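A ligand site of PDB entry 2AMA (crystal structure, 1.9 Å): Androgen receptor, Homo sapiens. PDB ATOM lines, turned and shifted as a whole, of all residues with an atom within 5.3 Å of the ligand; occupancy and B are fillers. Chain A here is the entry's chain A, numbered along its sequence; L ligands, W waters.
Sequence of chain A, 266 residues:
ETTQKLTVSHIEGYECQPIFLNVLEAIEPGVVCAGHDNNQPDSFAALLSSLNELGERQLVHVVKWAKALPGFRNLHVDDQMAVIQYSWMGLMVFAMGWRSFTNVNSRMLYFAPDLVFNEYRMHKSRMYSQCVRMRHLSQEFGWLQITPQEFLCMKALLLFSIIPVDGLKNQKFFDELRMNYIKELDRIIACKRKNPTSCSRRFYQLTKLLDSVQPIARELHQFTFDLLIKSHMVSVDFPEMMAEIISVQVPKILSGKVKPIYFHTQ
Merely in contact with the ligand: Leu 48 (3.9 Å), Leu 51 (3.3 Å), Leu 54 (3.97 Å), Met 89 (3.8 Å), Met 92 (3.8 Å), Met 96 (3.5 Å), Phe 111 (3.6 Å), Met 127 (3.6 Å), Phe 223 (3.8 Å), Phe 238 (3.8 Å) and Met 242 (3.7 Å). Hydrophobic or aromatic side chains that line the ligand: Leu 48, Leu 54, Met 89, Met 92, Met 96, Phe 111, Met 127, Phe 223, Phe 238 and Met 242. 14 residues have an atom within 4 Å of the ligand: Leu 48, Leu 51, Asn 52, Leu 54, Met 89, Met 92, Met 96, Arg 99, Phe 111, Met 127, Phe 223, Thr 224, Phe 238 and Met 242.
Water W1 lies within hydrogen-bond range of the backbone carbonyl oxygen of Met 92, the guanidinium group of Arg 99 and an oxygen (O1) of the ligand.
The backbone carbonyl oxygen (O) of Leu 48 lies close to the side-chain amide nitrogen (ND2) of Asn 52 (3.5 Å). The guanidinium group (NH2) of Arg 99 is in hydrogen-bond range of the backbone carbonyl oxygen (O) of Phe 111.
O2 of the ligand sits at hydrogen-bond distance from OD1 of Asn 52 (2.7 Å). The guanidinium group (NH2) of Arg 99 lies within hydrogen-bond range of an oxygen (O1) of the ligand. The side-chain hydroxyl (OG1) of Thr 224 is in hydrogen-bond range of an oxygen (O2) of the ligand.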
ATOM      1  N   LEU A  48      29.873 -28.245 -22.569  1.00  0.00           N
ATOM      2  CA  LEU A  48      29.755 -27.876 -23.975  1.00  0.00           C
ATOM      3  C   LEU A  48      28.305 -27.962 -24.461  1.00  0.00           C
ATOM      4  O   LEU A  48      27.861 -27.118 -25.239  1.00  0.00           O
ATOM      5  CB  LEU A  48      30.669 -28.757 -24.842  1.00  0.00           C
ATOM      6  CG  LEU A  48      32.087 -28.186 -25.029  1.00  0.00           C
ATOM      7  CD1 LEU A  48      32.006 -26.856 -25.800  1.00  0.00           C
ATOM      8  CD2 LEU A  48      32.749 -27.966 -23.679  1.00  0.00           C
ATOM      9  N   LEU A  51      26.753 -24.861 -23.333  1.00  0.00           N
ATOM     10  CA  LEU A  51      27.252 -23.720 -24.106  1.00  0.00           C
ATOM     11  C   LEU A  51      26.560 -23.673 -25.460  1.00  0.00           C
ATOM     12  O   LEU A  51      26.239 -22.582 -25.954  1.00  0.00           O
ATOM     13  CB  LEU A  51      28.767 -23.836 -24.308  1.00  0.00           C
ATOM     14  CG  LEU A  51      29.658 -23.426 -23.134  1.00  0.00           C
ATOM     15  CD1 LEU A  51      31.137 -23.693 -23.467  1.00  0.00           C
ATOM     16  CD2 LEU A  51      29.444 -21.947 -22.837  1.00  0.00           C
ATOM     17  N   ASN A  52      26.342 -24.842 -26.059  1.00  0.00           N
ATOM     18  CA  ASN A  52      25.681 -24.952 -27.358  1.00  0.00           C
ATOM     19  C   ASN A  52      24.224 -24.497 -27.253  1.00  0.00           C
ATOM     20  O   ASN A  52      23.706 -23.817 -28.139  1.00  0.00           O
ATOM     21  CB  ASN A  52      25.745 -26.386 -27.897  1.00  0.00           C
ATOM     22  CG  ASN A  52      27.117 -26.744 -28.477  1.00  0.00           C
ATOM     23  OD1 ASN A  52      27.886 -25.858 -28.870  1.00  0.00           O
ATOM     24  ND2 ASN A  52      27.418 -28.038 -28.545  1.00  0.00           N
ATOM     25  N   LEU A  54      23.113 -22.495 -24.963  1.00  0.00           N
ATOM     26  CA  LEU A  54      23.188 -21.065 -24.696  1.00  0.00           C
ATOM     27  C   LEU A  54      23.318 -20.345 -26.038  1.00  0.00           C
ATOM     28  O   LEU A  54      22.686 -19.311 -26.268  1.00  0.00           O
ATOM     29  CB  LEU A  54      24.388 -20.740 -23.819  1.00  0.00           C
ATOM     30  CG  LEU A  54      24.619 -19.241 -23.615  1.00  0.00           C
ATOM     31  CD1 LEU A  54      23.396 -18.605 -22.975  1.00  0.00           C
ATOM     32  CD2 LEU A  54      25.845 -19.034 -22.752  1.00  0.00           C
ATOM     33  N   GLY A  55      24.138 -20.910 -26.919  1.00  0.00           N
ATOM     34  CA  GLY A  55      24.328 -20.300 -28.223  1.00  0.00           C
ATOM     35  C   GLY A  55      23.040 -20.270 -29.030  1.00  0.00           C
ATOM     36  O   GLY A  55      22.752 -19.294 -29.707  1.00  0.00           O
ATOM     37  N   GLN A  58      20.889 -17.482 -27.528  1.00  0.00           N
ATOM     38  CA  GLN A  58      21.454 -16.174 -27.855  1.00  0.00           C
ATOM     39  C   GLN A  58      21.268 -15.836 -29.319  1.00  0.00           C
ATOM     40  O   GLN A  58      21.066 -14.676 -29.667  1.00  0.00           O
ATOM     41  CB  GLN A  58      22.962 -16.137 -27.525  1.00  0.00           C
ATOM     42  CG  GLN A  58      23.243 -15.965 -26.050  1.00  0.00           C
ATOM     43  CD  GLN A  58      23.082 -14.536 -25.609  1.00  0.00           C
ATOM     44  OE1 GLN A  58      22.428 -13.738 -26.281  1.00  0.00           O
ATOM     45  NE2 GLN A  58      23.688 -14.196 -24.483  1.00  0.00           N
ATOM     46  N   TRP A  88      28.043 -13.884 -35.723  1.00  0.00           N
ATOM     47  CA  TRP A  88      27.535 -14.270 -34.414  1.00  0.00           C
ATOM     48  C   TRP A  88      28.592 -14.671 -33.381  1.00  0.00           C
ATOM     49  O   TRP A  88      28.469 -14.321 -32.222  1.00  0.00           O
ATOM     50  CB  TRP A  88      26.478 -15.383 -34.513  1.00  0.00           C
ATOM     51  CG  TRP A  88      26.969 -16.719 -34.981  1.00  0.00           C
ATOM     52  CD1 TRP A  88      27.048 -17.156 -36.274  1.00  0.00           C
ATOM     53  CD2 TRP A  88      27.444 -17.800 -34.163  1.00  0.00           C
ATOM     54  NE1 TRP A  88      27.539 -18.442 -36.305  1.00  0.00           N
ATOM     55  CE2 TRP A  88      27.796 -18.856 -35.035  1.00  0.00           C
ATOM     56  CE3 TRP A  88      27.602 -17.973 -32.784  1.00  0.00           C
ATOM     57  CZ2 TRP A  88      28.301 -20.072 -34.555  1.00  0.00           C
ATOM     58  CZ3 TRP A  88      28.105 -19.185 -32.313  1.00  0.00           C
ATOM     59  CH2 TRP A  88      28.451 -20.216 -33.205  1.00  0.00           C
ATOM     60  N   MET A  89      29.635 -15.408 -33.779  1.00  0.00           N
ATOM     61  CA  MET A  89      30.641 -15.788 -32.794  1.00  0.00           C
ATOM     62  C   MET A  89      31.287 -14.555 -32.152  1.00  0.00           C
ATOM     63  O   MET A  89      31.336 -14.443 -30.922  1.00  0.00           O
ATOM     64  CB  MET A  89      31.725 -16.647 -33.425  1.00  0.00           C
ATOM     65  CG  MET A  89      32.692 -17.281 -32.406  1.00  0.00           C
ATOM     66  SD  MET A  89      31.895 -18.534 -31.364  1.00  0.00           S
ATOM     67  CE  MET A  89      31.877 -19.942 -32.525  1.00  0.00           C
ATOM     68  N   MET A  92      28.867 -12.556 -29.898  1.00  0.00           N
ATOM     69  CA  MET A  92      28.619 -13.189 -28.618  1.00  0.00           C
ATOM     70  C   MET A  92      29.839 -13.200 -27.710  1.00  0.00           C
ATOM     71  O   MET A  92      29.714 -13.077 -26.489  1.00  0.00           O
ATOM     72  CB  MET A  92      28.092 -14.610 -28.821  1.00  0.00           C
ATOM     73  CG  MET A  92      26.673 -14.650 -29.414  1.00  0.00           C
ATOM     74  SD  MET A  92      26.124 -16.350 -29.644  1.00  0.00           S
ATOM     75  CE  MET A  92      24.640 -16.099 -30.671  1.00  0.00           C
ATOM     76  N   VAL A  93      31.024 -13.358 -28.287  1.00  0.00           N
ATOM     77  CA  VAL A  93      32.223 -13.338 -27.462  1.00  0.00           C
ATOM     78  C   VAL A  93      32.394 -11.945 -26.862  1.00  0.00           C
ATOM     79  O   VAL A  93      32.667 -11.807 -25.660  1.00  0.00           O
ATOM     80  CB  VAL A  93      33.458 -13.715 -28.296  1.00  0.00           C
ATOM     81  CG1 VAL A  93      34.726 -13.492 -27.478  1.00  0.00           C
ATOM     82  CG2 VAL A  93      33.363 -15.195 -28.706  1.00  0.00           C
ATOM     83  N   MET A  96      29.873 -11.313 -24.123  1.00  0.00           N
ATOM     84  CA  MET A  96      30.196 -12.133 -22.965  1.00  0.00           C
ATOM     85  C   MET A  96      31.371 -11.525 -22.207  1.00  0.00           C
ATOM     86  O   MET A  96      31.425 -11.583 -20.980  1.00  0.00           O
ATOM     87  CB  MET A  96      30.511 -13.568 -23.393  1.00  0.00           C
ATOM     88  CG  MET A  96      30.743 -14.528 -22.229  1.00  0.00           C
ATOM     89  SD  MET A  96      32.390 -14.439 -21.485  1.00  0.00           S
ATOM     90  CE  MET A  96      33.383 -15.139 -22.819  1.00  0.00           C
ATOM     91  N   ARG A  99      29.884  -8.710 -20.196  1.00  0.00           N
ATOM     92  CA  ARG A  99      29.173  -9.233 -19.016  1.00  0.00           C
ATOM     93  C   ARG A  99      30.147  -9.646 -17.918  1.00  0.00           C
ATOM     94  O   ARG A  99      29.891  -9.416 -16.735  1.00  0.00           O
ATOM     95  CB  ARG A  99      28.346 -10.462 -19.389  1.00  0.00           C
ATOM     96  CG  ARG A  99      27.167 -10.205 -20.266  1.00  0.00           C
ATOM     97  CD  ARG A  99      26.180 -11.368 -20.188  1.00  0.00           C
ATOM     98  NE  ARG A  99      26.670 -12.600 -20.809  1.00  0.00           N
ATOM     99  CZ  ARG A  99      26.748 -12.792 -22.121  1.00  0.00           C
ATOM    100  NH1 ARG A  99      26.357 -11.838 -22.958  1.00  0.00           N
ATOM    101  NH2 ARG A  99      27.175 -13.950 -22.607  1.00  0.00           N
ATOM    102  N   PHE A 111      29.317 -16.511 -18.977  1.00  0.00           N
ATOM    103  CA  PHE A 111      28.554 -16.878 -20.177  1.00  0.00           C
ATOM    104  C   PHE A 111      27.075 -16.606 -19.953  1.00  0.00           C
ATOM    105  O   PHE A 111      26.382 -16.085 -20.837  1.00  0.00           O
ATOM    106  CB  PHE A 111      28.782 -18.353 -20.529  1.00  0.00           C
ATOM    107  CG  PHE A 111      30.165 -18.649 -21.027  1.00  0.00           C
ATOM    108  CD1 PHE A 111      31.118 -19.252 -20.204  1.00  0.00           C
ATOM    109  CD2 PHE A 111      30.536 -18.317 -22.336  1.00  0.00           C
ATOM    110  CE1 PHE A 111      32.396 -19.531 -20.665  1.00  0.00           C
ATOM    111  CE2 PHE A 111      31.813 -18.592 -22.805  1.00  0.00           C
ATOM    112  CZ  PHE A 111      32.753 -19.201 -21.972  1.00  0.00           C
ATOM    113  N   MET A 127      38.807 -26.003 -23.492  1.00  0.00           N
ATOM    114  CA  MET A 127      38.945 -24.767 -24.257  1.00  0.00           C
ATOM    115  C   MET A 127      39.722 -23.772 -23.415  1.00  0.00           C
ATOM    116  O   MET A 127      39.489 -22.562 -23.510  1.00  0.00           O
ATOM    117  CB  MET A 127      37.591 -24.124 -24.531  1.00  0.00           C
ATOM    118  CG  MET A 127      36.480 -25.050 -24.946  1.00  0.00           C
ATOM    119  SD  MET A 127      34.999 -24.056 -25.066  1.00  0.00           S
ATOM    120  CE  MET A 127      35.475 -22.997 -26.377  1.00  0.00           C
ATOM    121  N   MET A 134      39.696 -15.019 -24.114  1.00  0.00           N
ATOM    122  CA  MET A 134      38.429 -14.344 -23.840  1.00  0.00           C
ATOM    123  C   MET A 134      38.453 -13.545 -22.540  1.00  0.00           C
ATOM    124  O   MET A 134      37.896 -12.448 -22.463  1.00  0.00           O
ATOM    125  CB  MET A 134      37.265 -15.348 -23.834  1.00  0.00           C
ATOM    126  CG  MET A 134      36.900 -15.831 -25.227  1.00  0.00           C
ATOM    127  SD  MET A 134      35.406 -16.843 -25.289  1.00  0.00           S
ATOM    128  CE  MET A 134      36.033 -18.408 -24.771  1.00  0.00           C
ATOM    129  N   LEU A 220      37.521 -20.140 -32.014  1.00  0.00           N
ATOM    130  CA  LEU A 220      36.285 -20.774 -31.576  1.00  0.00           C
ATOM    131  C   LEU A 220      35.540 -21.405 -32.747  1.00  0.00           C
ATOM    132  O   LEU A 220      34.834 -22.396 -32.571  1.00  0.00           O
ATOM    133  CB  LEU A 220      35.400 -19.749 -30.860  1.00  0.00           C
ATOM    134  CG  LEU A 220      35.981 -19.303 -29.500  1.00  0.00           C
ATOM    135  CD1 LEU A 220      35.254 -18.068 -28.993  1.00  0.00           C
ATOM    136  CD2 LEU A 220      35.877 -20.447 -28.497  1.00  0.00           C
ATOM    137  N   PHE A 223      37.310 -24.667 -33.318  1.00  0.00           N
ATOM    138  CA  PHE A 223      36.968 -25.553 -32.207  1.00  0.00           C
ATOM    139  C   PHE A 223      35.546 -26.102 -32.311  1.00  0.00           C
ATOM    140  O   PHE A 223      35.328 -27.294 -32.138  1.00  0.00           O
ATOM    141  CB  PHE A 223      37.154 -24.815 -30.876  1.00  0.00           C
ATOM    142  CG  PHE A 223      36.965 -25.677 -29.669  1.00  0.00           C
ATOM    143  CD1 PHE A 223      35.698 -26.052 -29.249  1.00  0.00           C
ATOM    144  CD2 PHE A 223      38.069 -26.128 -28.936  1.00  0.00           C
ATOM    145  CE1 PHE A 223      35.521 -26.869 -28.135  1.00  0.00           C
ATOM    146  CE2 PHE A 223      37.894 -26.949 -27.813  1.00  0.00           C
ATOM    147  CZ  PHE A 223      36.623 -27.316 -27.411  1.00  0.00           C
ATOM    148  N   THR A 224      34.576 -25.231 -32.580  1.00  0.00           N
ATOM    149  CA  THR A 224      33.197 -25.687 -32.659  1.00  0.00           C
ATOM    150  C   THR A 224      33.000 -26.586 -33.885  1.00  0.00           C
ATOM    151  O   THR A 224      32.220 -27.535 -33.855  1.00  0.00           O
ATOM    152  CB  THR A 224      32.212 -24.491 -32.706  1.00  0.00           C
ATOM    153  OG1 THR A 224      30.880 -24.950 -32.414  1.00  0.00           O
ATOM    154  CG2 THR A 224      32.220 -23.850 -34.062  1.00  0.00           C
ATOM    155  N   LEU A 227      34.467 -29.923 -33.050  1.00  0.00           N
ATOM    156  CA  LEU A 227      33.577 -30.539 -32.072  1.00  0.00           C
ATOM    157  C   LEU A 227      32.283 -31.056 -32.722  1.00  0.00           C
ATOM    158  O   LEU A 227      31.767 -32.105 -32.339  1.00  0.00           O
ATOM    159  CB  LEU A 227      33.235 -29.553 -30.955  1.00  0.00           C
ATOM    160  CG  LEU A 227      32.354 -30.062 -29.806  1.00  0.00           C
ATOM    161  CD1 LEU A 227      32.957 -31.322 -29.207  1.00  0.00           C
ATOM    162  CD2 LEU A 227      32.211 -28.993 -28.742  1.00  0.00           C
ATOM    163  N   PHE A 238      24.329 -30.668 -30.235  1.00  0.00           N
ATOM    164  CA  PHE A 238      24.230 -29.382 -30.901  1.00  0.00           C
ATOM    165  C   PHE A 238      22.773 -29.156 -31.284  1.00  0.00           C
ATOM    166  O   PHE A 238      22.149 -30.030 -31.885  1.00  0.00           O
ATOM    167  CB  PHE A 238      25.054 -29.339 -32.180  1.00  0.00           C
ATOM    168  CG  PHE A 238      26.525 -29.166 -31.959  1.00  0.00           C
ATOM    169  CD1 PHE A 238      27.319 -30.246 -31.567  1.00  0.00           C
ATOM    170  CD2 PHE A 238      27.130 -27.924 -32.144  1.00  0.00           C
ATOM    171  CE1 PHE A 238      28.696 -30.090 -31.370  1.00  0.00           C
ATOM    172  CE2 PHE A 238      28.498 -27.757 -31.952  1.00  0.00           C
ATOM    173  CZ  PHE A 238      29.277 -28.835 -31.568  1.00  0.00           C
ATOM    174  N   MET A 242      22.353 -24.154 -34.501  1.00  0.00           N
ATOM    175  CA  MET A 242      23.800 -24.218 -34.342  1.00  0.00           C
ATOM    176  C   MET A 242      24.413 -25.221 -35.314  1.00  0.00           C
ATOM    177  O   MET A 242      25.363 -24.908 -36.030  1.00  0.00           O
ATOM    178  CB  MET A 242      24.147 -24.590 -32.889  1.00  0.00           C
ATOM    179  CG  MET A 242      23.839 -23.496 -31.862  1.00  0.00           C
ATOM    180  SD  MET A 242      24.901 -22.026 -32.033  1.00  0.00           S
ATOM    181  CE  MET A 242      26.324 -22.542 -31.097  1.00  0.00           C
ATOM    182  N   ILE A 246      26.936 -24.124 -38.271  1.00  0.00           N
ATOM    183  CA  ILE A 246      28.317 -24.558 -38.117  1.00  0.00           C
ATOM    184  C   ILE A 246      28.789 -25.461 -39.263  1.00  0.00           C
ATOM    185  O   ILE A 246      29.980 -25.496 -39.571  1.00  0.00           O
ATOM    186  CB  ILE A 246      28.523 -25.260 -36.760  1.00  0.00           C
ATOM    187  CG1 ILE A 246      28.169 -24.279 -35.632  1.00  0.00           C
ATOM    188  CG2 ILE A 246      29.978 -25.720 -36.609  1.00  0.00           C
ATOM    189  CD1 ILE A 246      28.252 -24.853 -34.227  1.00  0.00           C
HETATM  190  C1  LIG L   1      27.728 -18.865 -26.265  1.00  0.00           C
HETATM  191  C2  LIG L   1      27.400 -17.378 -26.013  1.00  0.00           C
HETATM  192  C3  LIG L   1      28.632 -16.755 -25.247  1.00  0.00           C
HETATM  193  O1  LIG L   1      28.299 -16.225 -24.177  1.00  0.00           O
HETATM  194  C4  LIG L   1      29.769 -16.891 -25.793  1.00  0.00           C
HETATM  195  C5  LIG L   1      30.192 -18.386 -26.033  1.00  0.00           C
HETATM  196  C6  LIG L   1      31.620 -18.540 -26.674  1.00  0.00           C
HETATM  197  C7  LIG L   1      31.952 -20.042 -26.845  1.00  0.00           C
HETATM  198  C8  LIG L   1      30.921 -20.776 -27.766  1.00  0.00           C
HETATM  199  C9  LIG L   1      29.480 -20.600 -27.158  1.00  0.00           C
HETATM  200  C10 LIG L   1      29.097 -19.072 -26.965  1.00  0.00           C
HETATM  201  C11 LIG L   1      28.483 -21.369 -28.068  1.00  0.00           C
HETATM  202  C12 LIG L   1      28.772 -22.845 -28.331  1.00  0.00           C
HETATM  203  C13 LIG L   1      30.228 -23.083 -28.826  1.00  0.00           C
HETATM  204  C14 LIG L   1      31.219 -22.300 -27.897  1.00  0.00           C
HETATM  205  C15 LIG L   1      32.583 -22.718 -28.482  1.00  0.00           C
HETATM  206  C16 LIG L   1      32.378 -24.245 -28.725  1.00  0.00           C
HETATM  207  C17 LIG L   1      30.841 -24.460 -28.653  1.00  0.00           C
HETATM  208  O2  LIG L   1      30.444 -25.392 -29.668  1.00  0.00           O
HETATM  209  C18 LIG L   1      30.329 -22.608 -30.333  1.00  0.00           C
HETATM  210  C19 LIG L   1      29.055 -18.377 -28.388  1.00  0.00           C
HETATM  211  O   HOH W   1      26.979 -13.520 -25.593  1.00  0.00           O
